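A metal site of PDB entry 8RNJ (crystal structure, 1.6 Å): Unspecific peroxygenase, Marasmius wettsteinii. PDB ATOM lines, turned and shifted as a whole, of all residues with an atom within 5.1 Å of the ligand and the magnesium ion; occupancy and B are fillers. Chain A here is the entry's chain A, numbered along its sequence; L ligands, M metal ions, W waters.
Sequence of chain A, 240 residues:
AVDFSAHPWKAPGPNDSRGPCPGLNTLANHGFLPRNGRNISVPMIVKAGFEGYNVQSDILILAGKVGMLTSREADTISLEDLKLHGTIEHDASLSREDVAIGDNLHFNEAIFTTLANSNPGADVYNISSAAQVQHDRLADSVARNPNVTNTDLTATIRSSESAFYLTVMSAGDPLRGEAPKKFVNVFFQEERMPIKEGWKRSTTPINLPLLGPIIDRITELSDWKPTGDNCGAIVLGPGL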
ATOM      1  N   PRO A  20      23.560   4.019  19.055  1.00  0.00           N
ATOM      2  CA  PRO A  20      22.703   3.044  18.379  1.00  0.00           C
ATOM      3  C   PRO A  20      21.325   2.827  19.017  1.00  0.00           C
ATOM      4  O   PRO A  20      20.536   2.015  18.539  1.00  0.00           O
ATOM      5  CB  PRO A  20      23.566   1.775  18.502  1.00  0.00           C
ATOM      6  CG  PRO A  20      24.200   1.912  19.866  1.00  0.00           C
ATOM      7  CD  PRO A  20      24.544   3.395  19.961  1.00  0.00           C
ATOM      8  N   CYS A  21      21.052   3.557  20.117  1.00  0.00           N
ATOM      9  CA  CYS A  21      19.825   3.435  20.883  1.00  0.00           C
ATOM     10  C   CYS A  21      18.861   4.560  20.548  1.00  0.00           C
ATOM     11  O   CYS A  21      19.098   5.708  20.923  1.00  0.00           O
ATOM     12  CB  CYS A  21      20.111   3.482  22.379  1.00  0.00           C
ATOM     13  SG  CYS A  21      18.601   3.436  23.378  1.00  0.00           S
ATOM     14  N   PRO A  22      17.690   4.265  19.937  1.00  0.00           N
ATOM     15  CA  PRO A  22      16.675   5.285  19.697  1.00  0.00           C
ATOM     16  C   PRO A  22      16.051   5.843  20.964  1.00  0.00           C
ATOM     17  O   PRO A  22      15.600   6.993  20.978  1.00  0.00           O
ATOM     18  CB  PRO A  22      15.619   4.566  18.830  1.00  0.00           C
ATOM     19  CG  PRO A  22      15.826   3.093  19.155  1.00  0.00           C
ATOM     20  CD  PRO A  22      17.304   2.947  19.428  1.00  0.00           C
ATOM     21  N   GLY A  23      16.017   5.049  22.040  1.00  0.00           N
ATOM     22  CA  GLY A  23      15.456   5.502  23.306  1.00  0.00           C
ATOM     23  C   GLY A  23      16.249   6.676  23.886  1.00  0.00           C
ATOM     24  O   GLY A  23      15.673   7.725  24.204  1.00  0.00           O
ATOM     25  N   LEU A  24      17.570   6.504  23.996  1.00  0.00           N
ATOM     26  CA  LEU A  24      18.408   7.551  24.575  1.00  0.00           C
ATOM     27  C   LEU A  24      18.579   8.699  23.572  1.00  0.00           C
ATOM     28  O   LEU A  24      18.584   9.864  23.979  1.00  0.00           O
ATOM     29  CB  LEU A  24      19.742   6.963  25.013  1.00  0.00           C
ATOM     30  CG  LEU A  24      19.660   5.878  26.088  1.00  0.00           C
ATOM     31  CD1 LEU A  24      21.072   5.392  26.411  1.00  0.00           C
ATOM     32  CD2 LEU A  24      18.954   6.368  27.351  1.00  0.00           C
ATOM     33  N   ILE A  45      20.324   9.283  33.278  1.00  0.00           N
ATOM     34  CA  ILE A  45      19.483   8.378  32.495  1.00  0.00           C
ATOM     35  C   ILE A  45      18.222   8.009  33.269  1.00  0.00           C
ATOM     36  O   ILE A  45      17.125   7.999  32.720  1.00  0.00           O
ATOM     37  CB  ILE A  45      20.283   7.136  32.074  1.00  0.00           C
ATOM     38  CG1 ILE A  45      21.357   7.515  31.055  1.00  0.00           C
ATOM     39  CG2 ILE A  45      19.352   6.056  31.547  1.00  0.00           C
ATOM     40  CD1 ILE A  45      22.333   6.393  30.757  1.00  0.00           C
ATOM     41  N   TYR A  53       9.453   8.996  29.556  1.00  0.00           N
ATOM     42  CA  TYR A  53       8.763   7.772  29.166  1.00  0.00           C
ATOM     43  C   TYR A  53       8.022   7.072  30.302  1.00  0.00           C
ATOM     44  O   TYR A  53       7.328   6.098  30.042  1.00  0.00           O
ATOM     45  CB  TYR A  53       9.758   6.746  28.600  1.00  0.00           C
ATOM     46  CG  TYR A  53      10.606   7.165  27.423  1.00  0.00           C
ATOM     47  CD1 TYR A  53      10.084   7.858  26.345  1.00  0.00           C
ATOM     48  CD2 TYR A  53      11.926   6.757  27.323  1.00  0.00           C
ATOM     49  CE1 TYR A  53      10.849   8.162  25.235  1.00  0.00           C
ATOM     50  CE2 TYR A  53      12.718   7.047  26.222  1.00  0.00           C
ATOM     51  CZ  TYR A  53      12.176   7.775  25.172  1.00  0.00           C
ATOM     52  OH  TYR A  53      12.962   8.061  24.094  1.00  0.00           O
ATOM     53  N   VAL A  55       9.644   5.293  32.398  1.00  0.00           N
ATOM     54  CA  VAL A  55      10.419   4.086  32.633  1.00  0.00           C
ATOM     55  C   VAL A  55      11.116   4.217  33.985  1.00  0.00           C
ATOM     56  O   VAL A  55      11.683   5.260  34.295  1.00  0.00           O
ATOM     57  CB  VAL A  55      11.408   3.793  31.495  1.00  0.00           C
ATOM     58  CG1 VAL A  55      12.356   2.626  31.822  1.00  0.00           C
ATOM     59  CG2 VAL A  55      10.675   3.508  30.180  1.00  0.00           C
ATOM     60  N   ILE A  59      15.116  -1.000  35.661  1.00  0.00           N
ATOM     61  CA  ILE A  59      15.691  -1.409  34.386  1.00  0.00           C
ATOM     62  C   ILE A  59      16.811  -0.441  33.982  1.00  0.00           C
ATOM     63  O   ILE A  59      17.794  -0.852  33.376  1.00  0.00           O
ATOM     64  CB  ILE A  59      14.640  -1.599  33.273  1.00  0.00           C
ATOM     65  CG1 ILE A  59      15.283  -1.999  31.935  1.00  0.00           C
ATOM     66  CG2 ILE A  59      13.797  -0.354  33.094  1.00  0.00           C
ATOM     67  CD1 ILE A  59      16.122  -3.266  31.968  1.00  0.00           C
ATOM     68  N   LEU A  60      16.646   0.856  34.262  1.00  0.00           N
ATOM     69  CA  LEU A  60      17.624   1.822  33.806  1.00  0.00           C
ATOM     70  C   LEU A  60      18.938   1.742  34.592  1.00  0.00           C
ATOM     71  O   LEU A  60      19.973   2.030  34.017  1.00  0.00           O
ATOM     72  CB  LEU A  60      17.025   3.230  33.869  1.00  0.00           C
ATOM     73  CG  LEU A  60      15.837   3.427  32.919  1.00  0.00           C
ATOM     74  CD1 LEU A  60      15.232   4.820  33.097  1.00  0.00           C
ATOM     75  CD2 LEU A  60      16.238   3.198  31.474  1.00  0.00           C
ATOM     76  N   ALA A  63      20.696  -1.589  33.069  1.00  0.00           N
ATOM     77  CA  ALA A  63      21.196  -1.359  31.726  1.00  0.00           C
ATOM     78  C   ALA A  63      22.197  -0.196  31.713  1.00  0.00           C
ATOM     79  O   ALA A  63      23.218  -0.289  31.029  1.00  0.00           O
ATOM     80  CB  ALA A  63      20.023  -1.093  30.815  1.00  0.00           C
ATOM     81  N   GLY A  64      21.924   0.848  32.494  1.00  0.00           N
ATOM     82  CA  GLY A  64      22.801   2.003  32.543  1.00  0.00           C
ATOM     83  C   GLY A  64      24.225   1.661  32.975  1.00  0.00           C
ATOM     84  O   GLY A  64      25.172   2.132  32.362  1.00  0.00           O
ATOM     85  N   GLY A  67      26.000  -0.064  30.304  1.00  0.00           N
ATOM     86  CA  GLY A  67      26.355   0.933  29.304  1.00  0.00           C
ATOM     87  C   GLY A  67      27.579   1.773  29.684  1.00  0.00           C
ATOM     88  O   GLY A  67      28.369   2.137  28.815  1.00  0.00           O
ATOM     89  N   LEU A  82      28.171   3.878  23.136  1.00  0.00           N
ATOM     90  CA  LEU A  82      27.337   2.695  23.284  1.00  0.00           C
ATOM     91  C   LEU A  82      27.346   1.799  22.049  1.00  0.00           C
ATOM     92  O   LEU A  82      26.822   0.673  22.100  1.00  0.00           O
ATOM     93  CB  LEU A  82      25.906   3.137  23.599  1.00  0.00           C
ATOM     94  CG  LEU A  82      25.660   3.733  24.983  1.00  0.00           C
ATOM     95  CD1 LEU A  82      24.242   4.304  25.056  1.00  0.00           C
ATOM     96  CD2 LEU A  82      25.829   2.680  26.075  1.00  0.00           C
ATOM     97  N   ILE A  88      26.622  -4.009  25.001  1.00  0.00           N
ATOM     98  CA  ILE A  88      25.195  -4.133  24.738  1.00  0.00           C
ATOM     99  C   ILE A  88      24.955  -4.291  23.235  1.00  0.00           C
ATOM    100  O   ILE A  88      24.183  -5.164  22.827  1.00  0.00           O
ATOM    101  CB  ILE A  88      24.417  -2.929  25.311  1.00  0.00           C
ATOM    102  CG1 ILE A  88      24.533  -2.843  26.841  1.00  0.00           C
ATOM    103  CG2 ILE A  88      22.954  -2.949  24.867  1.00  0.00           C
ATOM    104  CD1 ILE A  88      23.984  -1.590  27.463  1.00  0.00           C
ATOM    105  N   GLU A  89      25.628  -3.475  22.410  1.00  0.00           N
ATOM    106  CA  GLU A  89      25.420  -3.468  20.970  1.00  0.00           C
ATOM    107  C   GLU A  89      25.654  -4.873  20.386  1.00  0.00           C
ATOM    108  O   GLU A  89      26.614  -5.547  20.749  1.00  0.00           O
ATOM    109  CB  GLU A  89      26.303  -2.422  20.284  1.00  0.00           C
ATOM    110  CG  GLU A  89      25.896  -2.104  18.860  1.00  0.00           C
ATOM    111  CD  GLU A  89      26.258  -3.173  17.843  1.00  0.00           C
ATOM    112  OE1 GLU A  89      27.385  -3.670  17.910  1.00  0.00           O
ATOM    113  OE2 GLU A  89      25.427  -3.519  16.968  1.00  0.00           O
ATOM    114  N   HIS A  90      24.718  -5.306  19.536  1.00  0.00           N
ATOM    115  CA  HIS A  90      24.628  -6.685  19.062  1.00  0.00           C
ATOM    116  C   HIS A  90      24.260  -6.710  17.580  1.00  0.00           C
ATOM    117  O   HIS A  90      23.650  -5.774  17.051  1.00  0.00           O
ATOM    118  CB  HIS A  90      23.573  -7.452  19.876  1.00  0.00           C
ATOM    119  CG  HIS A  90      22.256  -6.754  19.892  1.00  0.00           C
ATOM    120  ND1 HIS A  90      21.421  -6.737  18.801  1.00  0.00           N
ATOM    121  CD2 HIS A  90      21.653  -6.017  20.840  1.00  0.00           C
ATOM    122  CE1 HIS A  90      20.379  -5.964  19.079  1.00  0.00           C
ATOM    123  NE2 HIS A  90      20.468  -5.560  20.310  1.00  0.00           N
ATOM    124  N   ASP A  91      24.532  -7.845  16.944  1.00  0.00           N
ATOM    125  CA  ASP A  91      24.026  -8.143  15.610  1.00  0.00           C
ATOM    126  C   ASP A  91      22.509  -8.342  15.592  1.00  0.00           C
ATOM    127  O   ASP A  91      21.872  -8.539  16.647  1.00  0.00           O
ATOM    128  CB  ASP A  91      24.712  -9.409  15.092  1.00  0.00           C
ATOM    129  CG  ASP A  91      26.235  -9.297  15.020  1.00  0.00           C
ATOM    130  OD1 ASP A  91      26.724  -8.187  14.773  1.00  0.00           O
ATOM    131  OD2 ASP A  91      26.950 -10.336  15.243  1.00  0.00           O
ATOM    132  N   SER A  93      20.142  -6.178  14.836  1.00  0.00           N
ATOM    133  CA  SER A  93      19.388  -5.002  15.260  1.00  0.00           C
ATOM    134  C   SER A  93      18.189  -4.769  14.348  1.00  0.00           C
ATOM    135  O   SER A  93      18.169  -5.239  13.211  1.00  0.00           O
ATOM    136  CB  SER A  93      20.267  -3.784  15.296  1.00  0.00           C
ATOM    137  OG  SER A  93      21.252  -3.897  16.315  1.00  0.00           O
ATOM    138  N   LEU A  94      17.235  -3.988  14.864  1.00  0.00           N
ATOM    139  CA  LEU A  94      15.983  -3.668  14.166  1.00  0.00           C
ATOM    140  C   LEU A  94      16.192  -2.596  13.085  1.00  0.00           C
ATOM    141  O   LEU A  94      15.411  -2.551  12.137  1.00  0.00           O
ATOM    142  CB  LEU A  94      14.967  -3.169  15.188  1.00  0.00           C
ATOM    143  CG  LEU A  94      14.539  -4.197  16.233  1.00  0.00           C
ATOM    144  CD1 LEU A  94      13.752  -3.539  17.347  1.00  0.00           C
ATOM    145  CD2 LEU A  94      13.714  -5.318  15.613  1.00  0.00           C
ATOM    146  N   SER A  95      17.168  -1.715  13.280  1.00  0.00           N
ATOM    147  CA  SER A  95      17.302  -0.528  12.434  1.00  0.00           C
ATOM    148  C   SER A  95      18.760  -0.178  12.107  1.00  0.00           C
ATOM    149  O   SER A  95      19.022   0.857  11.490  1.00  0.00           O
ATOM    150  CB  SER A  95      16.599   0.641  13.092  1.00  0.00           C
ATOM    151  OG  SER A  95      17.265   1.083  14.266  1.00  0.00           O
ATOM    152  N   ARG A  96      19.725  -1.011  12.552  1.00  0.00           N
ATOM    153  CA  ARG A  96      21.146  -0.833  12.285  1.00  0.00           C
ATOM    154  C   ARG A  96      21.706  -2.095  11.638  1.00  0.00           C
ATOM    155  O   ARG A  96      21.104  -3.157  11.747  1.00  0.00           O
ATOM    156  CB  ARG A  96      21.916  -0.578  13.594  1.00  0.00           C
ATOM    157  CG  ARG A  96      22.009   0.872  14.044  1.00  0.00           C
ATOM    158  CD  ARG A  96      20.696   1.528  14.399  1.00  0.00           C
ATOM    159  NE  ARG A  96      20.901   2.848  14.975  1.00  0.00           N
ATOM    160  CZ  ARG A  96      19.942   3.718  15.271  1.00  0.00           C
ATOM    161  NH1 ARG A  96      18.673   3.435  15.059  1.00  0.00           N
ATOM    162  NH2 ARG A  96      20.262   4.916  15.753  1.00  0.00           N
ATOM    163  N   GLU A  97      22.843  -1.954  10.939  1.00  0.00           N
ATOM    164  CA  GLU A  97      23.553  -3.064  10.320  1.00  0.00           C
ATOM    165  C   GLU A  97      24.495  -3.709  11.344  1.00  0.00           C
ATOM    166  O   GLU A  97      24.880  -3.063  12.319  1.00  0.00           O
ATOM    167  CB  GLU A  97      24.378  -2.600   9.125  1.00  0.00           C
ATOM    168  CG  GLU A  97      23.542  -1.932   8.041  1.00  0.00           C
ATOM    169  CD  GLU A  97      24.335  -1.376   6.873  1.00  0.00           C
ATOM    170  OE1 GLU A  97      25.325  -0.654   7.113  1.00  0.00           O
ATOM    171  OE2 GLU A  97      23.934  -1.661   5.717  1.00  0.00           O
ATOM    172  N   ASN A 104      27.010  -0.091  12.447  1.00  0.00           N
ATOM    173  CA  ASN A 104      26.246  -0.552  13.603  1.00  0.00           C
ATOM    174  C   ASN A 104      25.724   0.596  14.459  1.00  0.00           C
ATOM    175  O   ASN A 104      25.164   0.334  15.537  1.00  0.00           O
ATOM    176  CB  ASN A 104      27.057  -1.518  14.480  1.00  0.00           C
ATOM    177  CG  ASN A 104      28.133  -0.815  15.280  1.00  0.00           C
ATOM    178  OD1 ASN A 104      28.576   0.261  14.912  1.00  0.00           O
ATOM    179  ND2 ASN A 104      28.584  -1.423  16.371  1.00  0.00           N
ATOM    180  N   GLU A 161      14.550  -4.809  23.831  1.00  0.00           N
ATOM    181  CA  GLU A 161      14.448  -3.647  22.957  1.00  0.00           C
ATOM    182  C   GLU A 161      13.100  -3.641  22.238  1.00  0.00           C
ATOM    183  O   GLU A 161      12.461  -2.593  22.126  1.00  0.00           O
ATOM    184  CB  GLU A 161      15.682  -3.631  22.060  1.00  0.00           C
ATOM    185  CG  GLU A 161      16.925  -3.323  22.875  1.00  0.00           C
ATOM    186  CD  GLU A 161      18.289  -3.690  22.328  1.00  0.00           C
ATOM    187  OE1 GLU A 161      18.339  -4.310  21.272  1.00  0.00           O
ATOM    188  OE2 GLU A 161      19.296  -3.314  22.970  1.00  0.00           O
ATOM    189  N   PHE A 164      10.560  -2.585  24.666  1.00  0.00           N
ATOM    190  CA  PHE A 164      10.633  -1.154  24.872  1.00  0.00           C
ATOM    191  C   PHE A 164       9.812  -0.407  23.817  1.00  0.00           C
ATOM    192  O   PHE A 164       9.029   0.482  24.198  1.00  0.00           O
ATOM    193  CB  PHE A 164      12.081  -0.651  24.860  1.00  0.00           C
ATOM    194  CG  PHE A 164      12.715  -0.505  26.212  1.00  0.00           C
ATOM    195  CD1 PHE A 164      12.014   0.046  27.271  1.00  0.00           C
ATOM    196  CD2 PHE A 164      14.046  -0.842  26.408  1.00  0.00           C
ATOM    197  CE1 PHE A 164      12.601   0.232  28.508  1.00  0.00           C
ATOM    198  CE2 PHE A 164      14.640  -0.661  27.651  1.00  0.00           C
ATOM    199  CZ  PHE A 164      13.912  -0.134  28.697  1.00  0.00           C
ATOM    200  N   TYR A 165       9.954  -0.726  22.526  1.00  0.00           N
ATOM    201  CA  TYR A 165       9.224   0.056  21.530  1.00  0.00           C
ATOM    202  C   TYR A 165       7.726  -0.214  21.674  1.00  0.00           C
ATOM    203  O   TYR A 165       6.938   0.711  21.484  1.00  0.00           O
ATOM    204  CB  TYR A 165       9.772  -0.073  20.098  1.00  0.00           C
ATOM    205  CG  TYR A 165       9.416  -1.304  19.297  1.00  0.00           C
ATOM    206  CD1 TYR A 165       8.131  -1.534  18.817  1.00  0.00           C
ATOM    207  CD2 TYR A 165      10.416  -2.206  18.949  1.00  0.00           C
ATOM    208  CE1 TYR A 165       7.847  -2.659  18.059  1.00  0.00           C
ATOM    209  CE2 TYR A 165      10.146  -3.316  18.168  1.00  0.00           C
ATOM    210  CZ  TYR A 165       8.857  -3.543  17.717  1.00  0.00           C
ATOM    211  OH  TYR A 165       8.611  -4.672  16.984  1.00  0.00           O
ATOM    212  N   VAL A 168       6.833   1.840  25.482  1.00  0.00           N
ATOM    213  CA  VAL A 168       7.071   3.264  25.615  1.00  0.00           C
ATOM    214  C   VAL A 168       6.258   4.050  24.574  1.00  0.00           C
ATOM    215  O   VAL A 168       5.828   5.161  24.885  1.00  0.00           O
ATOM    216  CB  VAL A 168       8.569   3.588  25.533  1.00  0.00           C
ATOM    217  CG1 VAL A 168       8.838   5.062  25.453  1.00  0.00           C
ATOM    218  CG2 VAL A 168       9.344   2.979  26.707  1.00  0.00           C
ATOM    219  N   PHE A 187       9.431   7.277  16.153  1.00  0.00           N
ATOM    220  CA  PHE A 187      10.464   6.988  17.150  1.00  0.00           C
ATOM    221  C   PHE A 187      11.758   6.533  16.474  1.00  0.00           C
ATOM    222  O   PHE A 187      12.816   7.088  16.736  1.00  0.00           O
ATOM    223  CB  PHE A 187       9.875   5.973  18.145  1.00  0.00           C
ATOM    224  CG  PHE A 187      10.824   5.478  19.208  1.00  0.00           C
ATOM    225  CD1 PHE A 187      11.230   6.308  20.242  1.00  0.00           C
ATOM    226  CD2 PHE A 187      11.270   4.177  19.172  1.00  0.00           C
ATOM    227  CE1 PHE A 187      12.082   5.839  21.223  1.00  0.00           C
ATOM    228  CE2 PHE A 187      12.142   3.708  20.146  1.00  0.00           C
ATOM    229  CZ  PHE A 187      12.528   4.538  21.187  1.00  0.00           C
ATOM    230  N   PHE A 188      11.698   5.526  15.602  1.00  0.00           N
ATOM    231  CA  PHE A 188      12.882   5.014  14.931  1.00  0.00           C
ATOM    232  C   PHE A 188      13.416   5.965  13.854  1.00  0.00           C
ATOM    233  O   PHE A 188      14.608   6.239  13.811  1.00  0.00           O
ATOM    234  CB  PHE A 188      12.613   3.646  14.304  1.00  0.00           C
ATOM    235  CG  PHE A 188      12.698   2.471  15.248  1.00  0.00           C
ATOM    236  CD1 PHE A 188      13.908   1.849  15.491  1.00  0.00           C
ATOM    237  CD2 PHE A 188      11.545   1.977  15.853  1.00  0.00           C
ATOM    238  CE1 PHE A 188      13.974   0.772  16.369  1.00  0.00           C
ATOM    239  CE2 PHE A 188      11.617   0.896  16.718  1.00  0.00           C
ATOM    240  CZ  PHE A 188      12.827   0.283  16.950  1.00  0.00           C
HETATM  241  C1  LIG L   1      19.053  -0.393  21.385  1.00  0.00           C
HETATM  242  C2  LIG L   1      21.549   0.951  25.271  1.00  0.00           C
HETATM  243  C3  LIG L   1      17.488   2.648  27.251  1.00  0.00           C
HETATM  244  C4  LIG L   1      15.020   1.410  23.325  1.00  0.00           C
HETATM  245  C5  LIG L   1      20.079  -0.117  22.239  1.00  0.00           C
HETATM  246  C6  LIG L   1      21.420  -0.367  21.941  1.00  0.00           C
HETATM  247  C7  LIG L   1      22.150   0.042  23.009  1.00  0.00           C
HETATM  248  C8  LIG L   1      21.233   0.497  24.008  1.00  0.00           C
HETATM  249  C9  LIG L   1      23.646   0.000  23.149  1.00  0.00           C
HETATM  250  C10 LIG L   1      21.957  -0.909  20.647  1.00  0.00           C
HETATM  251  C11 LIG L   1      21.799  -2.427  20.604  1.00  0.00           C
HETATM  252  C12 LIG L   1      21.684  -2.927  19.193  1.00  0.00           C
HETATM  253  O1  LIG L   1      22.675  -3.427  18.661  1.00  0.00           O
HETATM  254  O2  LIG L   1      20.628  -2.813  18.563  1.00  0.00           O
HETATM  255  C13 LIG L   1      20.636   1.503  26.149  1.00  0.00           C
HETATM  256  C14 LIG L   1      20.992   1.952  27.455  1.00  0.00           C
HETATM  257  C15 LIG L   1      19.871   2.468  28.022  1.00  0.00           C
HETATM  258  C16 LIG L   1      18.782   2.244  27.026  1.00  0.00           C
HETATM  259  C17 LIG L   1      22.357   1.942  28.061  1.00  0.00           C
HETATM  260  C18 LIG L   1      19.640   2.978  29.410  1.00  0.00           C
HETATM  261  C19 LIG L   1      19.764   2.246  30.460  1.00  0.00           C
HETATM  262  C20 LIG L   1      16.452   2.509  26.362  1.00  0.00           C
HETATM  263  C21 LIG L   1      15.173   3.056  26.503  1.00  0.00           C
HETATM  264  C22 LIG L   1      14.447   2.691  25.397  1.00  0.00           C
HETATM  265  C23 LIG L   1      15.324   1.957  24.526  1.00  0.00           C
HETATM  266  C24 LIG L   1      14.644   3.840  27.692  1.00  0.00           C
HETATM  267  C25 LIG L   1      13.046   3.103  25.242  1.00  0.00           C
HETATM  268  C26 LIG L   1      12.354   3.066  24.158  1.00  0.00           C
HETATM  269  C27 LIG L   1      15.949   0.761  22.479  1.00  0.00           C
HETATM  270  C28 LIG L   1      15.565   0.116  21.213  1.00  0.00           C
HETATM  271  C29 LIG L   1      16.692  -0.377  20.664  1.00  0.00           C
HETATM  272  C30 LIG L   1      17.759  -0.053  21.640  1.00  0.00           C
HETATM  273  C31 LIG L   1      14.161   0.048  20.633  1.00  0.00           C
HETATM  274  C32 LIG L   1      16.815  -1.165  19.375  1.00  0.00           C
HETATM  275  C33 LIG L   1      17.481  -0.432  18.236  1.00  0.00           C
HETATM  276  C34 LIG L   1      17.651  -1.407  17.080  1.00  0.00           C
HETATM  277  O3  LIG L   1      17.887  -0.970  15.931  1.00  0.00           O
HETATM  278  O4  LIG L   1      17.511  -2.656  17.218  1.00  0.00           O
HETATM  279  N1  LIG L   1      19.966   0.425  23.521  1.00  0.00           N
HETATM  280  N2  LIG L   1      19.328   1.665  25.967  1.00  0.00           N
HETATM  281  N3  LIG L   1      16.545   1.891  25.146  1.00  0.00           N
HETATM  282  N4  LIG L   1      17.275   0.640  22.702  1.00  0.00           N
HETATM  283 FE1  LIG L   1      18.288   1.252  24.210  1.00  0.00          FE
HETATM  284 MG    MG M   1      23.433  -3.652  16.659  1.00  0.00          MG
HETATM  285  O   HOH W   1      23.716  -3.989  14.611  1.00  0.00           O
HETATM  286  O   HOH W   2      23.300  -1.572  16.454  1.00  0.00           O
HETATM  287  O   HOH W   3      21.034  -0.270  17.025  1.00  0.00           O
HETATM  288  O   HOH W   4      17.926  -0.801  25.137  1.00  0.00           O
HETATM  289  O   HOH W   5      17.337  -4.851  18.857  1.00  0.00           O
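The side-chain hydroxyl of Ser 95 lies within hydrogen-bond range of an oxygen (O3) of the ligand.
The side-chain sulfur (SG) of Cys 21 binds an iron atom (FE1) of the ligand (2.4 Å).
N of Ser 95 is in hydrogen-bond range of O3 of the ligand (2.8 Å).
N of His 90 sits close to O1 of the ligand (2.9 Å).
NE2 of His 90 lies close to O2 of the ligand (3.3 Å).
An oxygen (O4) of the ligand is in hydrogen-bond range of the backbone NH of Leu 94.
OG of Ser 95 sits at hydrogen-bond distance from NH1 of Arg 96 (2.9 Å).
The side-chain sulfur (SG) of Cys 21 lies close to the backbone NH (N) of Gly 23 (3.3 Å).
SG of Cys 21 sits close to N of Leu 24, at 3.3 Å.
ND2 of Asn 104 lies within hydrogen-bond range of OE1 of Glu 89 (3.0 Å).
OH of Tyr 53 is in hydrogen-bond range of O of Gly 23 (2.7 Å).
A ring nitrogen (NE2) of His 90 lies within hydrogen-bond range of the side-chain carboxylate (OE1) of Glu 161.
Residues that only touch the ligand: Gly 64, Phe 187, Glu 161, Ala 63, Leu 82, Ile 88, Leu 24, Leu 60, Pro 22, Phe 164, Gly 23, Pro 20, Ile 45, Arg 96, Phe 188 and Val 168.
Within 4 Å of the ligand: Pro 20, Cys 21, Pro 22, Gly 23, Leu 24, Ile 45, Leu 60, Ala 63, Gly 64, Leu 82, Ile 88, Glu 89, His 90, Ser 93, Leu 94, Ser 95, Arg 96, Glu 161, Phe 164, Val 168, Phe 187 and Phe 188.
The nearest printed residue that does not touch the ligand is Tyr 53 (4.004 Å).
Of the 30 residues printed, 3 come within 4 Å of the magnesium ion.
The magnesium ion is bound by the side-chain carboxylate of Glu 89 (2.0 Å), water W1 (2.1 Å), water W2 (2.1 Å), an oxygen (O1) of the ligand (2.2 Å), the backbone carbonyl oxygen of His 90 (2.2 Å) and the side-chain hydroxyl of Ser 93 (2.2 Å).
Water W5 bridges the side-chain carboxylate (OE1) of Glu 161 (2.7 Å) and an oxygen (O4) of the ligand (2.7 Å).
Water W3 lies within hydrogen-bond range of the backbone carbonyl oxygen of Pro 20 and an oxygen (O2) of the ligand.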
